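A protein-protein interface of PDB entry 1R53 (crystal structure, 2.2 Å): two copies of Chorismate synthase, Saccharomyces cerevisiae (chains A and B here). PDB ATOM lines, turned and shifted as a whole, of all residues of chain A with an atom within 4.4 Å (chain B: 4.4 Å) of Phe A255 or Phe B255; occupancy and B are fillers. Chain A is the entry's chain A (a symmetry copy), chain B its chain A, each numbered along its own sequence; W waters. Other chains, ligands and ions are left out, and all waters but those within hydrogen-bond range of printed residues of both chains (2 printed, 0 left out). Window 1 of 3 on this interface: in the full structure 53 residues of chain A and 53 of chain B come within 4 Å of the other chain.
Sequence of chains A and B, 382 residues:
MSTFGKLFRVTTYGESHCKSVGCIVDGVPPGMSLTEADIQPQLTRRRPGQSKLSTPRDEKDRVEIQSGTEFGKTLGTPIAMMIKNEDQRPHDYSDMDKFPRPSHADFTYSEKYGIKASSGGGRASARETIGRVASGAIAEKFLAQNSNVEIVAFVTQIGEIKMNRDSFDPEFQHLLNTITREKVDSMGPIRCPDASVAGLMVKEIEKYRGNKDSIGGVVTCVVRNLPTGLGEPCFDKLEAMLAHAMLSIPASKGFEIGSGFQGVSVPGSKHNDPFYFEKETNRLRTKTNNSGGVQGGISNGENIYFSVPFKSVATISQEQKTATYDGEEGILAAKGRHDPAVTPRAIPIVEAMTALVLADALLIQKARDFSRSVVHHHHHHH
Printed residues of chain A that touch a printed residue of chain B: Glu A239, Ala A243, Leu A247, Gly A254, Phe A255, Glu A256, Phe A261, Ser A307 and Pro A309.
Hydrophobic or aromatic side chains of chain A that line the printed part of chain B: Ala A243, Leu A247, Phe A255, Phe A261 and Pro A309.
Printed residues of chain B that touch a printed residue of chain A: Glu B239, Ala B243, Leu B247, Gly B254, Phe B255, Glu B256, Phe B261, Ser B307 and Pro B309.
Hydrophobic or aromatic side chains of chain B that line the printed part of chain A: Ala B243, Leu B247, Phe B255, Phe B261 and Pro B309.
Among the printed residues, no Asp or Glu carboxylate lies within 4 Å of a Lys or Arg side-chain nitrogen of the other chain.
Phe A255 touches three residues of chain B.
Phe B255 touches just these residues of chain A: Leu A247, Gly A254 and Phe A255.
Of the printed residues of chain B, Gly A254 touches Phe B255 (3.2 Å).
Printed residues of chain B within 4 Å of Ala A243: Leu B247 (3.5 Å).
Printed residues of chain A within 4 Å of Ser B307: Phe A261.
Of the printed residues of chain B, Leu A247 touches Glu B239 (3.7 Å), Ala B243 (3.5 Å) and Phe B255 (3.9 Å).
The nearest residue of chain A that does not touch Phe B255 is Phe A261 (4.2 Å).
Glu A239 touches Leu B247, and with the chains exchanged Leu A247 touches Glu B239.
Ala A243 touches Leu B247, and with the chains exchanged Leu A247 touches Ala B243.
Gly A254 touches Phe B255, and with the chains exchanged Phe A255 touches Gly B254.
Glu A256 touches Phe B261, and with the chains exchanged Phe A261 touches Glu B256.
Positions printed for both chains: 239, 242, 243, 246, 247, 254, 255, 256, 257, 261, 306, 307 and 309.
Of the 16 pairs that touch across the chains among the printed residues, 16 have their exchanged pair printed and touching as well.
OE1 of Glu B256 is in hydrogen-bond range of N of Phe B261 (2.9 Å).
O of Glu B256 sits at hydrogen-bond distance from N of Ser B307 (2.9 Å).
OE1 of Glu A256 is in hydrogen-bond range of N of Phe A261, at 2.9 Å.
O of Glu A256 is in hydrogen-bond range of N of Ser A307, at 2.9 Å.
Water W1 bridges OE2 of Glu A239 and O of Leu B247.
Water W2 bridges the side-chain carboxylate (OE2) of Glu B239 and the backbone carbonyl oxygen (O) of Leu A247.
The backbone carbonyl oxygen of Phe A255 sits at hydrogen-bond distance from the backbone NH of Phe B255 (2.9 Å).
Leu B247 touches Glu A239 (O to CG, 3.7 Å).
Leu A247 touches Ala B243.
Leu A247 touches Phe B255.
Gly B254 touches Phe A255 (CA to O, 3.2 Å).
CG of Glu A256 touches CZ of Phe B261, at 3.7 Å.
Phe A261 touches Glu B256.
Phe A261 touches Phe B261.
Pro B309 touches Phe A261.
Ser A307 touches Phe B261.
Pro A309 touches Phe B261 (CD to CZ, 3.5 Å).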
ATOM      1  N   GLU A 239       5.654  10.319  20.856  1.00  0.00           N
ATOM      2  CA  GLU A 239       6.096  11.685  20.647  1.00  0.00           C
ATOM      3  C   GLU A 239       4.923  12.670  20.788  1.00  0.00           C
ATOM      4  O   GLU A 239       5.130  13.822  21.137  1.00  0.00           O
ATOM      5  CB  GLU A 239       6.800  11.855  19.302  1.00  0.00           C
ATOM      6  CG  GLU A 239       5.997  11.507  18.059  1.00  0.00           C
ATOM      7  CD  GLU A 239       6.297  10.097  17.553  1.00  0.00           C
ATOM      8  OE1 GLU A 239       6.212   9.117  18.336  1.00  0.00           O
ATOM      9  OE2 GLU A 239       6.648   9.973  16.379  1.00  0.00           O
ATOM     10  N   LEU A 242       4.389  12.957  24.500  1.00  0.00           N
ATOM     11  CA  LEU A 242       5.417  13.843  25.036  1.00  0.00           C
ATOM     12  C   LEU A 242       5.148  15.317  24.699  1.00  0.00           C
ATOM     13  O   LEU A 242       5.389  16.198  25.557  1.00  0.00           O
ATOM     14  CB  LEU A 242       6.812  13.444  24.582  1.00  0.00           C
ATOM     15  CG  LEU A 242       7.394  12.187  25.201  1.00  0.00           C
ATOM     16  CD1 LEU A 242       8.537  11.671  24.342  1.00  0.00           C
ATOM     17  CD2 LEU A 242       7.816  12.354  26.655  1.00  0.00           C
ATOM     18  N   ALA A 243       4.601  15.579  23.501  1.00  0.00           N
ATOM     19  CA  ALA A 243       4.441  16.945  23.042  1.00  0.00           C
ATOM     20  C   ALA A 243       3.307  17.604  23.800  1.00  0.00           C
ATOM     21  O   ALA A 243       3.364  18.766  24.212  1.00  0.00           O
ATOM     22  CB  ALA A 243       4.180  16.944  21.546  1.00  0.00           C
ATOM     23  N   MET A 246       4.696  18.544  27.145  1.00  0.00           N
ATOM     24  CA  MET A 246       5.621  19.661  27.200  1.00  0.00           C
ATOM     25  C   MET A 246       4.969  21.010  26.906  1.00  0.00           C
ATOM     26  O   MET A 246       5.361  22.051  27.499  1.00  0.00           O
ATOM     27  CB  MET A 246       6.776  19.415  26.272  1.00  0.00           C
ATOM     28  CG  MET A 246       7.720  18.239  26.693  1.00  0.00           C
ATOM     29  SD  MET A 246       8.064  17.936  28.467  1.00  0.00           S
ATOM     30  CE  MET A 246       7.922  16.608  28.404  1.00  0.00           C
ATOM     31  N   LEU A 247       3.976  21.007  26.011  1.00  0.00           N
ATOM     32  CA  LEU A 247       3.260  22.227  25.670  1.00  0.00           C
ATOM     33  C   LEU A 247       2.360  22.678  26.783  1.00  0.00           C
ATOM     34  O   LEU A 247       1.993  23.810  26.831  1.00  0.00           O
ATOM     35  CB  LEU A 247       2.572  22.093  24.279  1.00  0.00           C
ATOM     36  CG  LEU A 247       3.738  22.625  23.446  1.00  0.00           C
ATOM     37  CD1 LEU A 247       4.426  21.668  22.482  1.00  0.00           C
ATOM     38  CD2 LEU A 247       3.619  24.102  23.014  1.00  0.00           C
ATOM     39  N   GLY A 254       6.946  25.174  22.426  1.00  0.00           N
ATOM     40  CA  GLY A 254       7.195  24.151  21.438  1.00  0.00           C
ATOM     41  C   GLY A 254       7.753  22.846  21.940  1.00  0.00           C
ATOM     42  O   GLY A 254       7.874  22.632  23.116  1.00  0.00           O
ATOM     43  N   PHE A 255       8.033  21.958  20.994  1.00  0.00           N
ATOM     44  CA  PHE A 255       8.498  20.632  21.244  1.00  0.00           C
ATOM     45  C   PHE A 255       9.101  20.091  19.926  1.00  0.00           C
ATOM     46  O   PHE A 255       8.525  20.293  18.851  1.00  0.00           O
ATOM     47  CB  PHE A 255       7.403  19.739  21.735  1.00  0.00           C
ATOM     48  CG  PHE A 255       7.802  18.287  21.821  1.00  0.00           C
ATOM     49  CD1 PHE A 255       8.290  17.757  22.976  1.00  0.00           C
ATOM     50  CD2 PHE A 255       7.668  17.458  20.738  1.00  0.00           C
ATOM     51  CE1 PHE A 255       8.667  16.421  23.060  1.00  0.00           C
ATOM     52  CE2 PHE A 255       8.054  16.136  20.806  1.00  0.00           C
ATOM     53  CZ  PHE A 255       8.554  15.613  22.002  1.00  0.00           C
ATOM     54  N   GLU A 256      10.278  19.476  20.001  1.00  0.00           N
ATOM     55  CA  GLU A 256      10.808  18.767  18.858  1.00  0.00           C
ATOM     56  C   GLU A 256      11.571  17.567  19.329  1.00  0.00           C
ATOM     57  O   GLU A 256      12.190  17.582  20.405  1.00  0.00           O
ATOM     58  CB  GLU A 256      11.658  19.655  17.987  1.00  0.00           C
ATOM     59  CG  GLU A 256      12.855  20.192  18.695  1.00  0.00           C
ATOM     60  CD  GLU A 256      13.947  20.670  17.761  1.00  0.00           C
ATOM     61  OE1 GLU A 256      13.652  21.221  16.693  1.00  0.00           O
ATOM     62  OE2 GLU A 256      15.109  20.493  18.129  1.00  0.00           O
ATOM     63  N   ILE A 257      11.505  16.516  18.543  1.00  0.00           N
ATOM     64  CA  ILE A 257      12.126  15.249  18.901  1.00  0.00           C
ATOM     65  C   ILE A 257      13.110  14.834  17.829  1.00  0.00           C
ATOM     66  O   ILE A 257      12.882  15.043  16.642  1.00  0.00           O
ATOM     67  CB  ILE A 257      11.056  14.159  19.153  1.00  0.00           C
ATOM     68  CG1 ILE A 257      11.717  12.855  19.594  1.00  0.00           C
ATOM     69  CG2 ILE A 257      10.203  13.896  17.933  1.00  0.00           C
ATOM     70  CD1 ILE A 257      10.788  11.919  20.335  1.00  0.00           C
ATOM     71  N   PHE A 261      13.622  20.365  13.918  1.00  0.00           N
ATOM     72  CA  PHE A 261      13.605  21.482  12.998  1.00  0.00           C
ATOM     73  C   PHE A 261      14.920  21.584  12.235  1.00  0.00           C
ATOM     74  O   PHE A 261      14.941  21.942  11.050  1.00  0.00           O
ATOM     75  CB  PHE A 261      13.322  22.830  13.730  1.00  0.00           C
ATOM     76  CG  PHE A 261      11.863  23.058  13.961  1.00  0.00           C
ATOM     77  CD1 PHE A 261      11.041  23.483  12.938  1.00  0.00           C
ATOM     78  CD2 PHE A 261      11.284  22.761  15.173  1.00  0.00           C
ATOM     79  CE1 PHE A 261       9.689  23.646  13.141  1.00  0.00           C
ATOM     80  CE2 PHE A 261       9.940  22.924  15.368  1.00  0.00           C
ATOM     81  CZ  PHE A 261       9.141  23.374  14.332  1.00  0.00           C
ATOM     82  N   PHE A 306      14.587  15.211  23.163  1.00  0.00           N
ATOM     83  CA  PHE A 306      13.754  16.277  22.644  1.00  0.00           C
ATOM     84  C   PHE A 306      14.080  17.611  23.274  1.00  0.00           C
ATOM     85  O   PHE A 306      14.765  17.686  24.283  1.00  0.00           O
ATOM     86  CB  PHE A 306      12.268  15.920  22.849  1.00  0.00           C
ATOM     87  CG  PHE A 306      11.877  15.739  24.290  1.00  0.00           C
ATOM     88  CD1 PHE A 306      11.520  16.819  25.060  1.00  0.00           C
ATOM     89  CD2 PHE A 306      11.914  14.495  24.884  1.00  0.00           C
ATOM     90  CE1 PHE A 306      11.183  16.672  26.333  1.00  0.00           C
ATOM     91  CE2 PHE A 306      11.557  14.354  26.188  1.00  0.00           C
ATOM     92  CZ  PHE A 306      11.170  15.454  26.909  1.00  0.00           C
ATOM     93  N   SER A 307      13.612  18.683  22.653  1.00  0.00           N
ATOM     94  CA  SER A 307      13.883  20.022  23.146  1.00  0.00           C
ATOM     95  C   SER A 307      12.622  20.833  23.183  1.00  0.00           C
ATOM     96  O   SER A 307      11.728  20.669  22.362  1.00  0.00           O
ATOM     97  CB  SER A 307      14.937  20.749  22.288  1.00  0.00           C
ATOM     98  OG  SER A 307      16.186  20.084  22.338  1.00  0.00           O
ATOM     99  N   PRO A 309      11.372  25.026  23.787  1.00  0.00           N
ATOM    100  CA  PRO A 309      11.673  26.452  23.970  1.00  0.00           C
ATOM    101  C   PRO A 309      10.730  27.061  25.017  1.00  0.00           C
ATOM    102  O   PRO A 309       9.557  26.671  25.102  1.00  0.00           O
ATOM    103  CB  PRO A 309      11.390  27.056  22.576  1.00  0.00           C
ATOM    104  CG  PRO A 309      10.270  26.146  21.986  1.00  0.00           C
ATOM    105  CD  PRO A 309      10.320  24.836  22.779  1.00  0.00           C
ATOM    106  N   GLU B 239      -2.613  24.839  23.003  1.00  0.00           N
ATOM    107  CA  GLU B 239      -1.362  24.569  22.319  1.00  0.00           C
ATOM    108  C   GLU B 239      -0.907  23.119  22.557  1.00  0.00           C
ATOM    109  O   GLU B 239      -0.209  22.553  21.730  1.00  0.00           O
ATOM    110  CB  GLU B 239      -0.271  25.561  22.717  1.00  0.00           C
ATOM    111  CG  GLU B 239       0.094  25.625  24.191  1.00  0.00           C
ATOM    112  CD  GLU B 239      -0.614  26.770  24.913  1.00  0.00           C
ATOM    113  OE1 GLU B 239      -1.863  26.887  24.833  1.00  0.00           O
ATOM    114  OE2 GLU B 239       0.084  27.573  25.533  1.00  0.00           O
ATOM    115  N   LEU B 242      -3.092  21.072  20.278  1.00  0.00           N
ATOM    116  CA  LEU B 242      -2.565  21.192  18.922  1.00  0.00           C
ATOM    117  C   LEU B 242      -1.279  20.377  18.724  1.00  0.00           C
ATOM    118  O   LEU B 242      -1.098  19.769  17.643  1.00  0.00           O
ATOM    119  CB  LEU B 242      -2.339  22.641  18.521  1.00  0.00           C
ATOM    120  CG  LEU B 242      -3.578  23.472  18.249  1.00  0.00           C
ATOM    121  CD1 LEU B 242      -3.234  24.951  18.324  1.00  0.00           C
ATOM    122  CD2 LEU B 242      -4.279  23.125  16.943  1.00  0.00           C
ATOM    123  N   ALA B 243      -0.432  20.309  19.763  1.00  0.00           N
ATOM    124  CA  ALA B 243       0.866  19.679  19.621  1.00  0.00           C
ATOM    125  C   ALA B 243       0.696  18.176  19.551  1.00  0.00           C
ATOM    126  O   ALA B 243       1.336  17.466  18.772  1.00  0.00           O
ATOM    127  CB  ALA B 243       1.749  20.083  20.790  1.00  0.00           C
ATOM    128  N   MET B 246      -0.419  17.414  16.062  1.00  0.00           N
ATOM    129  CA  MET B 246       0.564  17.532  15.001  1.00  0.00           C
ATOM    130  C   MET B 246       1.659  16.470  15.061  1.00  0.00           C
ATOM    131  O   MET B 246       2.155  16.004  13.999  1.00  0.00           O
ATOM    132  CB  MET B 246       1.159  18.911  15.006  1.00  0.00           C
ATOM    133  CG  MET B 246       0.169  20.057  14.609  1.00  0.00           C
ATOM    134  SD  MET B 246      -1.104  19.759  13.325  1.00  0.00           S
ATOM    135  CE  MET B 246      -2.102  20.348  13.990  1.00  0.00           C
ATOM    136  N   LEU B 247       2.037  16.074  16.281  1.00  0.00           N
ATOM    137  CA  LEU B 247       3.051  15.047  16.464  1.00  0.00           C
ATOM    138  C   LEU B 247       2.543  13.685  16.094  1.00  0.00           C
ATOM    139  O   LEU B 247       3.311  12.813  15.834  1.00  0.00           O
ATOM    140  CB  LEU B 247       3.690  15.150  17.880  1.00  0.00           C
ATOM    141  CG  LEU B 247       4.822  16.105  17.502  1.00  0.00           C
ATOM    142  CD1 LEU B 247       4.814  17.503  18.106  1.00  0.00           C
ATOM    143  CD2 LEU B 247       6.196  15.441  17.271  1.00  0.00           C
ATOM    144  N   GLY B 254       7.973  17.672  15.167  1.00  0.00           N
ATOM    145  CA  GLY B 254       7.851  18.777  16.088  1.00  0.00           C
ATOM    146  C   GLY B 254       6.643  19.662  15.928  1.00  0.00           C
ATOM    147  O   GLY B 254       5.771  19.389  15.150  1.00  0.00           O
ATOM    148  N   PHE B 255       6.604  20.706  16.748  1.00  0.00           N
ATOM    149  CA  PHE B 255       5.519  21.631  16.824  1.00  0.00           C
ATOM    150  C   PHE B 255       6.034  22.895  17.553  1.00  0.00           C
ATOM    151  O   PHE B 255       6.754  22.786  18.552  1.00  0.00           O
ATOM    152  CB  PHE B 255       4.338  21.051  17.535  1.00  0.00           C
ATOM    153  CG  PHE B 255       3.248  22.055  17.813  1.00  0.00           C
ATOM    154  CD1 PHE B 255       2.213  22.231  16.946  1.00  0.00           C
ATOM    155  CD2 PHE B 255       3.265  22.809  18.958  1.00  0.00           C
ATOM    156  CE1 PHE B 255       1.208  23.161  17.193  1.00  0.00           C
ATOM    157  CE2 PHE B 255       2.284  23.745  19.204  1.00  0.00           C
ATOM    158  CZ  PHE B 255       1.231  23.910  18.300  1.00  0.00           C
ATOM    159  N   GLU B 256       5.729  24.074  17.018  1.00  0.00           N
ATOM    160  CA  GLU B 256       5.993  25.297  17.743  1.00  0.00           C
ATOM    161  C   GLU B 256       4.921  26.298  17.435  1.00  0.00           C
ATOM    162  O   GLU B 256       4.374  26.329  16.320  1.00  0.00           O
ATOM    163  CB  GLU B 256       7.363  25.846  17.442  1.00  0.00           C
ATOM    164  CG  GLU B 256       7.546  26.203  16.007  1.00  0.00           C
ATOM    165  CD  GLU B 256       8.686  27.170  15.763  1.00  0.00           C
ATOM    166  OE1 GLU B 256       9.718  27.095  16.442  1.00  0.00           O
ATOM    167  OE2 GLU B 256       8.529  27.998  14.865  1.00  0.00           O
ATOM    168  N   ILE B 257       4.595  27.095  18.427  1.00  0.00           N
ATOM    169  CA  ILE B 257       3.517  28.067  18.310  1.00  0.00           C
ATOM    170  C   ILE B 257       4.042  29.458  18.586  1.00  0.00           C
ATOM    171  O   ILE B 257       4.899  29.657  19.441  1.00  0.00           O
ATOM    172  CB  ILE B 257       2.338  27.701  19.244  1.00  0.00           C
ATOM    173  CG1 ILE B 257       1.187  28.688  19.062  1.00  0.00           C
ATOM    174  CG2 ILE B 257       2.744  27.674  20.700  1.00  0.00           C
ATOM    175  CD1 ILE B 257      -0.153  28.154  19.517  1.00  0.00           C
ATOM    176  N   PHE B 261      10.784  28.623  18.671  1.00  0.00           N
ATOM    177  CA  PHE B 261      12.205  28.414  18.849  1.00  0.00           C
ATOM    178  C   PHE B 261      12.992  29.673  18.504  1.00  0.00           C
ATOM    179  O   PHE B 261      14.004  29.984  19.143  1.00  0.00           O
ATOM    180  CB  PHE B 261      12.727  27.222  17.991  1.00  0.00           C
ATOM    181  CG  PHE B 261      12.498  25.900  18.651  1.00  0.00           C
ATOM    182  CD1 PHE B 261      13.311  25.470  19.679  1.00  0.00           C
ATOM    183  CD2 PHE B 261      11.415  25.121  18.317  1.00  0.00           C
ATOM    184  CE1 PHE B 261      13.068  24.274  20.317  1.00  0.00           C
ATOM    185  CE2 PHE B 261      11.178  23.935  18.955  1.00  0.00           C
ATOM    186  CZ  PHE B 261      12.023  23.515  19.967  1.00  0.00           C
ATOM    187  N   PHE B 306       1.278  28.248  13.931  1.00  0.00           N
ATOM    188  CA  PHE B 306       2.265  27.282  14.369  1.00  0.00           C
ATOM    189  C   PHE B 306       2.949  26.602  13.206  1.00  0.00           C
ATOM    190  O   PHE B 306       2.502  26.680  12.072  1.00  0.00           O
ATOM    191  CB  PHE B 306       1.600  26.246  15.298  1.00  0.00           C
ATOM    192  CG  PHE B 306       0.496  25.460  14.646  1.00  0.00           C
ATOM    193  CD1 PHE B 306       0.778  24.331  13.916  1.00  0.00           C
ATOM    194  CD2 PHE B 306      -0.815  25.879  14.724  1.00  0.00           C
ATOM    195  CE1 PHE B 306      -0.185  23.636  13.329  1.00  0.00           C
ATOM    196  CE2 PHE B 306      -1.797  25.153  14.126  1.00  0.00           C
ATOM    197  CZ  PHE B 306      -1.475  24.011  13.439  1.00  0.00           C
ATOM    198  N   SER B 307       4.069  25.952  13.483  1.00  0.00           N
ATOM    199  CA  SER B 307       4.832  25.282  12.444  1.00  0.00           C
ATOM    200  C   SER B 307       5.203  23.895  12.877  1.00  0.00           C
ATOM    201  O   SER B 307       5.429  23.626  14.050  1.00  0.00           O
ATOM    202  CB  SER B 307       6.109  26.063  12.073  1.00  0.00           C
ATOM    203  OG  SER B 307       5.793  27.333  11.531  1.00  0.00           O
ATOM    204  N   PRO B 309       7.804  20.575  11.561  1.00  0.00           N
ATOM    205  CA  PRO B 309       8.830  20.010  10.677  1.00  0.00           C
ATOM    206  C   PRO B 309       8.477  18.560  10.315  1.00  0.00           C
ATOM    207  O   PRO B 309       7.917  17.830  11.143  1.00  0.00           O
ATOM    208  CB  PRO B 309      10.108  20.049  11.547  1.00  0.00           C
ATOM    209  CG  PRO B 309       9.581  19.893  13.005  1.00  0.00           C
ATOM    210  CD  PRO B 309       8.097  20.275  12.968  1.00  0.00           C
HETATM  211  O   HOH W   1       4.679  10.651  14.131  1.00  0.00           O
HETATM  212  O   HOH W   2       1.647  26.633  27.995  1.00  0.00           O
